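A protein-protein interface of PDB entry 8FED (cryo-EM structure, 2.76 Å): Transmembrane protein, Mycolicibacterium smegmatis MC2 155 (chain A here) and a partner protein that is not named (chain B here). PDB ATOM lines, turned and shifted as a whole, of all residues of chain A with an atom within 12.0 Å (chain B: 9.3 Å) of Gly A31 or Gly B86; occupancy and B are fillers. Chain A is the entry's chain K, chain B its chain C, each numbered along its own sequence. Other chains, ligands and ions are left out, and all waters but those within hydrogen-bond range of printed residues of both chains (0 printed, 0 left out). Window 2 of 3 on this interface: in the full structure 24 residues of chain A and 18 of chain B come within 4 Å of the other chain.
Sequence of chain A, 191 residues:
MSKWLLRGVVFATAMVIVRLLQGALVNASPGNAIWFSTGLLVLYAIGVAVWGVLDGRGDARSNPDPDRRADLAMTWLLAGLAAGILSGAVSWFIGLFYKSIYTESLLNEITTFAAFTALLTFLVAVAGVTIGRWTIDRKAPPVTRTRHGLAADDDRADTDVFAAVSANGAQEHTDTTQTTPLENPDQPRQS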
ATOM      1  N   GLN A  22      13.391   4.845 -12.359  1.00  0.00           N
ATOM      2  CA  GLN A  22      14.226   3.728 -12.783  1.00  0.00           C
ATOM      3  C   GLN A  22      14.250   2.633 -11.730  1.00  0.00           C
ATOM      4  O   GLN A  22      14.179   1.447 -12.065  1.00  0.00           O
ATOM      5  CB  GLN A  22      15.644   4.210 -13.083  1.00  0.00           C
ATOM      6  CG  GLN A  22      16.566   3.122 -13.603  1.00  0.00           C
ATOM      7  CD  GLN A  22      17.879   3.064 -12.851  1.00  0.00           C
ATOM      8  OE1 GLN A  22      18.009   3.617 -11.760  1.00  0.00           O
ATOM      9  NE2 GLN A  22      18.863   2.388 -13.433  1.00  0.00           N
ATOM     10  N   GLY A  23      14.361   3.006 -10.455  1.00  0.00           N
ATOM     11  CA  GLY A  23      14.324   2.007  -9.401  1.00  0.00           C
ATOM     12  C   GLY A  23      13.012   1.249  -9.377  1.00  0.00           C
ATOM     13  O   GLY A  23      12.996   0.020  -9.260  1.00  0.00           O
ATOM     14  N   ALA A  24      11.894   1.973  -9.506  1.00  0.00           N
ATOM     15  CA  ALA A  24      10.591   1.313  -9.537  1.00  0.00           C
ATOM     16  C   ALA A  24      10.476   0.365 -10.727  1.00  0.00           C
ATOM     17  O   ALA A  24       9.986  -0.763 -10.584  1.00  0.00           O
ATOM     18  CB  ALA A  24       9.475   2.357  -9.573  1.00  0.00           C
ATOM     19  N   LEU A  25      10.931   0.798 -11.906  1.00  0.00           N
ATOM     20  CA  LEU A  25      10.818  -0.040 -13.098  1.00  0.00           C
ATOM     21  C   LEU A  25      11.719  -1.267 -13.011  1.00  0.00           C
ATOM     22  O   LEU A  25      11.329  -2.357 -13.443  1.00  0.00           O
ATOM     23  CB  LEU A  25      11.137   0.775 -14.350  1.00  0.00           C
ATOM     24  CG  LEU A  25      10.135   1.868 -14.728  1.00  0.00           C
ATOM     25  CD1 LEU A  25      10.556   2.561 -16.012  1.00  0.00           C
ATOM     26  CD2 LEU A  25       8.734   1.294 -14.858  1.00  0.00           C
ATOM     27  N   VAL A  26      12.934  -1.108 -12.477  1.00  0.00           N
ATOM     28  CA  VAL A  26      13.840  -2.244 -12.341  1.00  0.00           C
ATOM     29  C   VAL A  26      13.294  -3.243 -11.331  1.00  0.00           C
ATOM     30  O   VAL A  26      13.356  -4.461 -11.548  1.00  0.00           O
ATOM     31  CB  VAL A  26      15.254  -1.764 -11.962  1.00  0.00           C
ATOM     32  CG1 VAL A  26      16.155  -2.946 -11.653  1.00  0.00           C
ATOM     33  CG2 VAL A  26      15.858  -0.949 -13.091  1.00  0.00           C
ATOM     34  N   ASN A  27      12.749  -2.754 -10.213  1.00  0.00           N
ATOM     35  CA  ASN A  27      12.132  -3.658  -9.248  1.00  0.00           C
ATOM     36  C   ASN A  27      10.930  -4.380  -9.846  1.00  0.00           C
ATOM     37  O   ASN A  27      10.720  -5.569  -9.580  1.00  0.00           O
ATOM     38  CB  ASN A  27      11.724  -2.888  -7.993  1.00  0.00           C
ATOM     39  CG  ASN A  27      12.917  -2.425  -7.184  1.00  0.00           C
ATOM     40  OD1 ASN A  27      14.045  -2.410  -7.674  1.00  0.00           O
ATOM     41  ND2 ASN A  27      12.672  -2.042  -5.935  1.00  0.00           N
ATOM     42  N   ALA A  28      10.124  -3.680 -10.649  1.00  0.00           N
ATOM     43  CA  ALA A  28       8.951  -4.319 -11.242  1.00  0.00           C
ATOM     44  C   ALA A  28       9.341  -5.390 -12.255  1.00  0.00           C
ATOM     45  O   ALA A  28       8.858  -6.526 -12.186  1.00  0.00           O
ATOM     46  CB  ALA A  28       8.056  -3.263 -11.893  1.00  0.00           C
ATOM     47  N   SER A  29      10.213  -5.051 -13.205  1.00  0.00           N
ATOM     48  CA  SER A  29      10.597  -5.961 -14.286  1.00  0.00           C
ATOM     49  C   SER A  29      12.110  -5.952 -14.446  1.00  0.00           C
ATOM     50  O   SER A  29      12.655  -5.159 -15.226  1.00  0.00           O
ATOM     51  CB  SER A  29       9.909  -5.579 -15.595  1.00  0.00           C
ATOM     52  OG  SER A  29      10.353  -6.399 -16.662  1.00  0.00           O
ATOM     53  N   PRO A  30      12.826  -6.815 -13.720  1.00  0.00           N
ATOM     54  CA  PRO A  30      14.295  -6.822 -13.830  1.00  0.00           C
ATOM     55  C   PRO A  30      14.822  -7.197 -15.207  1.00  0.00           C
ATOM     56  O   PRO A  30      15.887  -6.693 -15.594  1.00  0.00           O
ATOM     57  CB  PRO A  30      14.719  -7.853 -12.776  1.00  0.00           C
ATOM     58  CG  PRO A  30      13.559  -7.949 -11.837  1.00  0.00           C
ATOM     59  CD  PRO A  30      12.344  -7.746 -12.687  1.00  0.00           C
ATOM     60  N   GLY A  31      14.044  -7.924 -16.014  1.00  0.00           N
ATOM     61  CA  GLY A  31      14.559  -8.398 -17.292  1.00  0.00           C
ATOM     62  C   GLY A  31      14.856  -7.261 -18.246  1.00  0.00           C
ATOM     63  O   GLY A  31      15.879  -7.269 -18.934  1.00  0.00           O
ATOM     64  N   ASN A  32      13.974  -6.274 -18.301  1.00  0.00           N
ATOM     65  CA  ASN A  32      14.134  -5.159 -19.212  1.00  0.00           C
ATOM     66  C   ASN A  32      14.806  -3.992 -18.509  1.00  0.00           C
ATOM     67  O   ASN A  32      14.851  -2.888 -19.066  1.00  0.00           O
ATOM     68  CB  ASN A  32      12.779  -4.731 -19.778  1.00  0.00           C
ATOM     69  CG  ASN A  32      12.003  -5.890 -20.366  1.00  0.00           C
ATOM     70  OD1 ASN A  32      12.580  -6.802 -20.956  1.00  0.00           O
ATOM     71  ND2 ASN A  32      10.685  -5.862 -20.205  1.00  0.00           N
ATOM     72  N   ALA A  33      15.364  -4.244 -17.313  1.00  0.00           N
ATOM     73  CA  ALA A  33      15.810  -3.171 -16.428  1.00  0.00           C
ATOM     74  C   ALA A  33      16.742  -2.198 -17.138  1.00  0.00           C
ATOM     75  O   ALA A  33      16.481  -0.988 -17.175  1.00  0.00           O
ATOM     76  CB  ALA A  33      16.501  -3.774 -15.204  1.00  0.00           C
ATOM     77  N   ILE A  34      17.793  -2.730 -17.771  1.00  0.00           N
ATOM     78  CA  ILE A  34      18.781  -1.892 -18.448  1.00  0.00           C
ATOM     79  C   ILE A  34      18.095  -0.978 -19.452  1.00  0.00           C
ATOM     80  O   ILE A  34      18.290   0.245 -19.438  1.00  0.00           O
ATOM     81  CB  ILE A  34      19.862  -2.766 -19.113  1.00  0.00           C
ATOM     82  CG1 ILE A  34      20.672  -1.958 -20.134  1.00  0.00           C
ATOM     83  CG2 ILE A  34      19.250  -4.016 -19.740  1.00  0.00           C
ATOM     84  CD1 ILE A  34      21.528  -0.866 -19.525  1.00  0.00           C
ATOM     85  N   TRP A  35      17.215  -1.557 -20.280  1.00  0.00           N
ATOM     86  CA  TRP A  35      16.483  -0.778 -21.271  1.00  0.00           C
ATOM     87  C   TRP A  35      15.784   0.401 -20.618  1.00  0.00           C
ATOM     88  O   TRP A  35      15.989   1.555 -21.020  1.00  0.00           O
ATOM     89  CB  TRP A  35      15.475  -1.666 -22.001  1.00  0.00           C
ATOM     90  CG  TRP A  35      16.113  -2.663 -22.913  1.00  0.00           C
ATOM     91  CD1 TRP A  35      16.362  -3.975 -22.646  1.00  0.00           C
ATOM     92  CD2 TRP A  35      16.591  -2.425 -24.241  1.00  0.00           C
ATOM     93  NE1 TRP A  35      16.964  -4.572 -23.727  1.00  0.00           N
ATOM     94  CE2 TRP A  35      17.115  -3.641 -24.719  1.00  0.00           C
ATOM     95  CE3 TRP A  35      16.624  -1.302 -25.074  1.00  0.00           C
ATOM     96  CZ2 TRP A  35      17.667  -3.767 -25.992  1.00  0.00           C
ATOM     97  CZ3 TRP A  35      17.173  -1.428 -26.337  1.00  0.00           C
ATOM     98  CH2 TRP A  35      17.686  -2.652 -26.784  1.00  0.00           C
ATOM     99  N   PHE A  36      15.024   0.128 -19.549  1.00  0.00           N
ATOM    100  CA  PHE A  36      14.316   1.190 -18.842  1.00  0.00           C
ATOM    101  C   PHE A  36      15.272   2.312 -18.476  1.00  0.00           C
ATOM    102  O   PHE A  36      15.049   3.475 -18.843  1.00  0.00           O
ATOM    103  CB  PHE A  36      13.632   0.631 -17.593  1.00  0.00           C
ATOM    104  CG  PHE A  36      12.379  -0.143 -17.882  1.00  0.00           C
ATOM    105  CD1 PHE A  36      11.514   0.262 -18.884  1.00  0.00           C
ATOM    106  CD2 PHE A  36      12.067  -1.277 -17.152  1.00  0.00           C
ATOM    107  CE1 PHE A  36      10.359  -0.448 -19.151  1.00  0.00           C
ATOM    108  CE2 PHE A  36      10.913  -1.992 -17.416  1.00  0.00           C
ATOM    109  CZ  PHE A  36      10.059  -1.576 -18.417  1.00  0.00           C
ATOM    110  N   SER A  37      16.396   1.954 -17.842  1.00  0.00           N
ATOM    111  CA  SER A  37      17.376   2.953 -17.436  1.00  0.00           C
ATOM    112  C   SER A  37      17.786   3.805 -18.626  1.00  0.00           C
ATOM    113  O   SER A  37      17.630   5.034 -18.607  1.00  0.00           O
ATOM    114  CB  SER A  37      18.593   2.270 -16.810  1.00  0.00           C
ATOM    115  OG  SER A  37      19.529   3.226 -16.344  1.00  0.00           O
ATOM    116  N   THR A  38      18.206   3.144 -19.712  1.00  0.00           N
ATOM    117  CA  THR A  38      18.646   3.871 -20.898  1.00  0.00           C
ATOM    118  C   THR A  38      17.547   4.798 -21.386  1.00  0.00           C
ATOM    119  O   THR A  38      17.785   5.995 -21.604  1.00  0.00           O
ATOM    120  CB  THR A  38      19.059   2.894 -21.999  1.00  0.00           C
ATOM    121  OG1 THR A  38      17.958   2.035 -22.317  1.00  0.00           O
ATOM    122  CG2 THR A  38      20.240   2.052 -21.546  1.00  0.00           C
ATOM    123  N   GLY A  39      16.318   4.278 -21.467  1.00  0.00           N
ATOM    124  CA  GLY A  39      15.204   5.103 -21.898  1.00  0.00           C
ATOM    125  C   GLY A  39      15.078   6.354 -21.061  1.00  0.00           C
ATOM    126  O   GLY A  39      15.080   7.472 -21.588  1.00  0.00           O
ATOM    127  N   TYR A 102      18.977   2.719  -6.090  1.00  0.00           N
ATOM    128  CA  TYR A 102      20.277   2.058  -6.165  1.00  0.00           C
ATOM    129  C   TYR A 102      21.344   3.120  -5.913  1.00  0.00           C
ATOM    130  O   TYR A 102      21.854   3.744  -6.846  1.00  0.00           O
ATOM    131  CB  TYR A 102      20.464   1.369  -7.512  1.00  0.00           C
ATOM    132  CG  TYR A 102      19.490   0.239  -7.753  1.00  0.00           C
ATOM    133  CD1 TYR A 102      18.240   0.477  -8.311  1.00  0.00           C
ATOM    134  CD2 TYR A 102      19.816  -1.067  -7.415  1.00  0.00           C
ATOM    135  CE1 TYR A 102      17.347  -0.554  -8.528  1.00  0.00           C
ATOM    136  CE2 TYR A 102      18.929  -2.104  -7.628  1.00  0.00           C
ATOM    137  CZ  TYR A 102      17.697  -1.841  -8.185  1.00  0.00           C
ATOM    138  OH  TYR A 102      16.812  -2.871  -8.399  1.00  0.00           O
ATOM    139  N   ALA B  38      21.983  -0.900 -13.477  1.00  0.00           N
ATOM    140  CA  ALA B  38      21.370  -1.240 -12.201  1.00  0.00           C
ATOM    141  C   ALA B  38      20.607  -2.546 -12.342  1.00  0.00           C
ATOM    142  O   ALA B  38      19.791  -2.698 -13.257  1.00  0.00           O
ATOM    143  CB  ALA B  38      20.431  -0.134 -11.718  1.00  0.00           C
ATOM    144  N   VAL B  39      20.873  -3.480 -11.436  1.00  0.00           N
ATOM    145  CA  VAL B  39      20.154  -4.748 -11.370  1.00  0.00           C
ATOM    146  C   VAL B  39      19.754  -4.982  -9.918  1.00  0.00           C
ATOM    147  O   VAL B  39      20.427  -4.474  -9.010  1.00  0.00           O
ATOM    148  CB  VAL B  39      21.006  -5.905 -11.916  1.00  0.00           C
ATOM    149  CG1 VAL B  39      21.118  -5.814 -13.428  1.00  0.00           C
ATOM    150  CG2 VAL B  39      22.385  -5.884 -11.283  1.00  0.00           C
ATOM    151  N   PRO B  40      18.663  -5.701  -9.650  1.00  0.00           N
ATOM    152  CA  PRO B  40      18.294  -5.986  -8.258  1.00  0.00           C
ATOM    153  C   PRO B  40      19.368  -6.804  -7.558  1.00  0.00           C
ATOM    154  O   PRO B  40      20.022  -7.656  -8.163  1.00  0.00           O
ATOM    155  CB  PRO B  40      16.983  -6.768  -8.390  1.00  0.00           C
ATOM    156  CG  PRO B  40      16.447  -6.387  -9.726  1.00  0.00           C
ATOM    157  CD  PRO B  40      17.649  -6.192 -10.597  1.00  0.00           C
ATOM    158  N   THR B  41      19.550  -6.530  -6.270  1.00  0.00           N
ATOM    159  CA  THR B  41      20.558  -7.194  -5.454  1.00  0.00           C
ATOM    160  C   THR B  41      19.861  -8.101  -4.449  1.00  0.00           C
ATOM    161  O   THR B  41      19.043  -7.636  -3.650  1.00  0.00           O
ATOM    162  CB  THR B  41      21.438  -6.171  -4.735  1.00  0.00           C
ATOM    163  OG1 THR B  41      22.173  -5.410  -5.701  1.00  0.00           O
ATOM    164  CG2 THR B  41      22.410  -6.865  -3.798  1.00  0.00           C
ATOM    165  N   TYR B  42      20.191  -9.385  -4.492  1.00  0.00           N
ATOM    166  CA  TYR B  42      19.650 -10.367  -3.566  1.00  0.00           C
ATOM    167  C   TYR B  42      20.687 -10.695  -2.500  1.00  0.00           C
ATOM    168  O   TYR B  42      21.867 -10.365  -2.623  1.00  0.00           O
ATOM    169  CB  TYR B  42      19.213 -11.629  -4.316  1.00  0.00           C
ATOM    170  CG  TYR B  42      18.278 -11.345  -5.468  1.00  0.00           C
ATOM    171  CD1 TYR B  42      16.923 -11.142  -5.251  1.00  0.00           C
ATOM    172  CD2 TYR B  42      18.751 -11.272  -6.769  1.00  0.00           C
ATOM    173  CE1 TYR B  42      16.064 -10.879  -6.299  1.00  0.00           C
ATOM    174  CE2 TYR B  42      17.901 -11.008  -7.824  1.00  0.00           C
ATOM    175  CZ  TYR B  42      16.559 -10.813  -7.583  1.00  0.00           C
ATOM    176  OH  TYR B  42      15.709 -10.551  -8.631  1.00  0.00           O
ATOM    177  N   ILE B  60      24.341 -19.841 -12.300  1.00  0.00           N
ATOM    178  CA  ILE B  60      23.175 -20.714 -12.251  1.00  0.00           C
ATOM    179  C   ILE B  60      23.354 -21.768 -13.330  1.00  0.00           C
ATOM    180  O   ILE B  60      23.581 -21.430 -14.497  1.00  0.00           O
ATOM    181  CB  ILE B  60      21.867 -19.933 -12.460  1.00  0.00           C
ATOM    182  CG1 ILE B  60      21.715 -18.848 -11.398  1.00  0.00           C
ATOM    183  CG2 ILE B  60      20.679 -20.874 -12.428  1.00  0.00           C
ATOM    184  CD1 ILE B  60      20.458 -18.033 -11.546  1.00  0.00           C
ATOM    185  N   VAL B  65      25.863 -15.691 -14.068  1.00  0.00           N
ATOM    186  CA  VAL B  65      24.680 -14.835 -14.086  1.00  0.00           C
ATOM    187  C   VAL B  65      24.920 -13.545 -13.312  1.00  0.00           C
ATOM    188  O   VAL B  65      24.150 -12.589 -13.447  1.00  0.00           O
ATOM    189  CB  VAL B  65      23.441 -15.568 -13.536  1.00  0.00           C
ATOM    190  CG1 VAL B  65      23.277 -16.931 -14.187  1.00  0.00           C
ATOM    191  CG2 VAL B  65      23.515 -15.694 -12.026  1.00  0.00           C
ATOM    192  N   GLY B  66      25.972 -13.489 -12.505  1.00  0.00           N
ATOM    193  CA  GLY B  66      26.225 -12.257 -11.782  1.00  0.00           C
ATOM    194  C   GLY B  66      27.515 -12.308 -10.995  1.00  0.00           C
ATOM    195  O   GLY B  66      28.336 -13.207 -11.164  1.00  0.00           O
ATOM    196  N   ASN B  67      27.672 -11.321 -10.115  1.00  0.00           N
ATOM    197  CA  ASN B  67      28.856 -11.180  -9.281  1.00  0.00           C
ATOM    198  C   ASN B  67      28.453 -10.975  -7.827  1.00  0.00           C
ATOM    199  O   ASN B  67      27.311 -10.626  -7.517  1.00  0.00           O
ATOM    200  CB  ASN B  67      29.737 -10.005  -9.734  1.00  0.00           C
ATOM    201  CG  ASN B  67      30.592 -10.340 -10.939  1.00  0.00           C
ATOM    202  OD1 ASN B  67      30.278 -11.245 -11.710  1.00  0.00           O
ATOM    203  ND2 ASN B  67      31.686  -9.608 -11.105  1.00  0.00           N
ATOM    204  N   TYR B  82      24.583 -10.318  -3.617  1.00  0.00           N
ATOM    205  CA  TYR B  82      25.030 -10.565  -4.979  1.00  0.00           C
ATOM    206  C   TYR B  82      23.956 -10.078  -5.942  1.00  0.00           C
ATOM    207  O   TYR B  82      22.889  -9.610  -5.534  1.00  0.00           O
ATOM    208  CB  TYR B  82      25.338 -12.053  -5.193  1.00  0.00           C
ATOM    209  CG  TYR B  82      24.211 -12.973  -4.776  1.00  0.00           C
ATOM    210  CD1 TYR B  82      23.189 -13.297  -5.657  1.00  0.00           C
ATOM    211  CD2 TYR B  82      24.170 -13.515  -3.499  1.00  0.00           C
ATOM    212  CE1 TYR B  82      22.158 -14.130  -5.279  1.00  0.00           C
ATOM    213  CE2 TYR B  82      23.142 -14.351  -3.112  1.00  0.00           C
ATOM    214  CZ  TYR B  82      22.139 -14.655  -4.007  1.00  0.00           C
ATOM    215  OH  TYR B  82      21.114 -15.488  -3.630  1.00  0.00           O
ATOM    216  N   THR B  83      24.246 -10.182  -7.237  1.00  0.00           N
ATOM    217  CA  THR B  83      23.307  -9.815  -8.285  1.00  0.00           C
ATOM    218  C   THR B  83      23.134 -10.986  -9.238  1.00  0.00           C
ATOM    219  O   THR B  83      24.065 -11.761  -9.465  1.00  0.00           O
ATOM    220  CB  THR B  83      23.775  -8.578  -9.066  1.00  0.00           C
ATOM    221  OG1 THR B  83      25.063  -8.830  -9.639  1.00  0.00           O
ATOM    222  CG2 THR B  83      23.856  -7.367  -8.155  1.00  0.00           C
ATOM    223  N   LEU B  84      21.930 -11.111  -9.793  1.00  0.00           N
ATOM    224  CA  LEU B  84      21.614 -12.181 -10.729  1.00  0.00           C
ATOM    225  C   LEU B  84      21.550 -11.707 -12.174  1.00  0.00           C
ATOM    226  O   LEU B  84      21.196 -12.494 -13.056  1.00  0.00           O
ATOM    227  CB  LEU B  84      20.294 -12.845 -10.343  1.00  0.00           C
ATOM    228  CG  LEU B  84      20.310 -13.689  -9.071  1.00  0.00           C
ATOM    229  CD1 LEU B  84      18.947 -14.299  -8.844  1.00  0.00           C
ATOM    230  CD2 LEU B  84      21.373 -14.767  -9.157  1.00  0.00           C
ATOM    231  N   GLY B  85      21.894 -10.451 -12.439  1.00  0.00           N
ATOM    232  CA  GLY B  85      21.903  -9.950 -13.806  1.00  0.00           C
ATOM    233  C   GLY B  85      20.542  -9.918 -14.464  1.00  0.00           C
ATOM    234  O   GLY B  85      20.411 -10.301 -15.634  1.00  0.00           O
ATOM    235  N   GLY B  86      19.520  -9.471 -13.740  1.00  0.00           N
ATOM    236  CA  GLY B  86      18.185  -9.387 -14.295  1.00  0.00           C
ATOM    237  C   GLY B  86      17.411 -10.683 -14.313  1.00  0.00           C
ATOM    238  O   GLY B  86      16.304 -10.715 -14.860  1.00  0.00           O
ATOM    239  N   ARG B  87      17.952 -11.752 -13.740  1.00  0.00           N
ATOM    240  CA  ARG B  87      17.273 -13.036 -13.711  1.00  0.00           C
ATOM    241  C   ARG B  87      16.463 -13.188 -12.426  1.00  0.00           C
ATOM    242  O   ARG B  87      16.616 -12.431 -11.466  1.00  0.00           O
ATOM    243  CB  ARG B  87      18.280 -14.175 -13.852  1.00  0.00           C
ATOM    244  CG  ARG B  87      18.918 -14.243 -15.223  1.00  0.00           C
ATOM    245  CD  ARG B  87      19.981 -15.317 -15.296  1.00  0.00           C
ATOM    246  NE  ARG B  87      20.481 -15.479 -16.655  1.00  0.00           N
ATOM    247  CZ  ARG B  87      21.425 -14.727 -17.200  1.00  0.00           C
ATOM    248  NH1 ARG B  87      21.999 -13.742 -16.528  1.00  0.00           N
ATOM    249  NH2 ARG B  87      21.805 -14.968 -18.451  1.00  0.00           N
ATOM    250  N   THR B  88      15.586 -14.188 -12.422  1.00  0.00           N
ATOM    251  CA  THR B  88      14.683 -14.442 -11.308  1.00  0.00           C
ATOM    252  C   THR B  88      14.822 -15.889 -10.865  1.00  0.00           C
ATOM    253  O   THR B  88      14.790 -16.801 -11.697  1.00  0.00           O
ATOM    254  CB  THR B  88      13.231 -14.144 -11.704  1.00  0.00           C
ATOM    255  OG1 THR B  88      13.079 -12.740 -11.948  1.00  0.00           O
ATOM    256  CG2 THR B  88      12.272 -14.570 -10.606  1.00  0.00           C
ATOM    257  N   ILE B  89      14.979 -16.096  -9.558  1.00  0.00           N
ATOM    258  CA  ILE B  89      15.054 -17.429  -8.978  1.00  0.00           C
ATOM    259  C   ILE B  89      13.960 -17.558  -7.929  1.00  0.00           C
ATOM    260  O   ILE B  89      13.439 -16.569  -7.408  1.00  0.00           O
ATOM    261  CB  ILE B  89      16.431 -17.730  -8.354  1.00  0.00           C
ATOM    262  CG1 ILE B  89      16.741 -16.732  -7.237  1.00  0.00           C
ATOM    263  CG2 ILE B  89      17.510 -17.707  -9.416  1.00  0.00           C
ATOM    264  CD1 ILE B  89      18.040 -17.007  -6.517  1.00  0.00           C
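Of the 17 printed residues of chain B, 4 touch a printed residue of chain A. Hydrophobic or aromatic side chains of chain B within 4 Å of the printed part of chain A: Ala B38 and Pro B40.
Among the printed residues, pairs that only touch across the chains: Tyr A102 with Val B39, Gln A22 with Ala B38, Tyr A102 with Pro B40, Val A26 with Pro B40, Pro A30 with Gly B86, Gly A31 with Gly B86, Pro A30 with Pro B40, Ala A33 with Ala B38 and Val A26 with Ala B38.
Of the printed residues of chain B, Gln A22 touches Ala B38 (3.4 Å). Of the printed residues of chain B, Val A26 touches Ala B38 and Pro B40. Pro A30 touches just these residues of chain B: Pro B40 (3.8 Å) and Gly B86 (3.8 Å). Gly A31 touches just one residue of chain B: Gly B86. Val B39 touches just one residue of chain A: Tyr A102. Pro B40 touches just these residues of chain A: Val A26, Pro A30 and Tyr A102. No residue of chain A comes within 4 Å of Leu B84. Of chain A, only Pro A30 (3.8 Å) and Gly A31 (3.8 Å) come within 4 Å of Gly B86. No residue of chain A comes within 4 Å of Thr B88. The nearest residue of chain B that does not touch Gly A31 is Arg B87 (5.9 Å).
NE2 of Gln A22 lies within hydrogen-bond range of OG of Ser A37, at 3.1 Å. The side-chain amide oxygen (OD1) of Asn A27 lies within hydrogen-bond range of the side-chain hydroxyl (OH) of Tyr A102 (2.9 Å).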
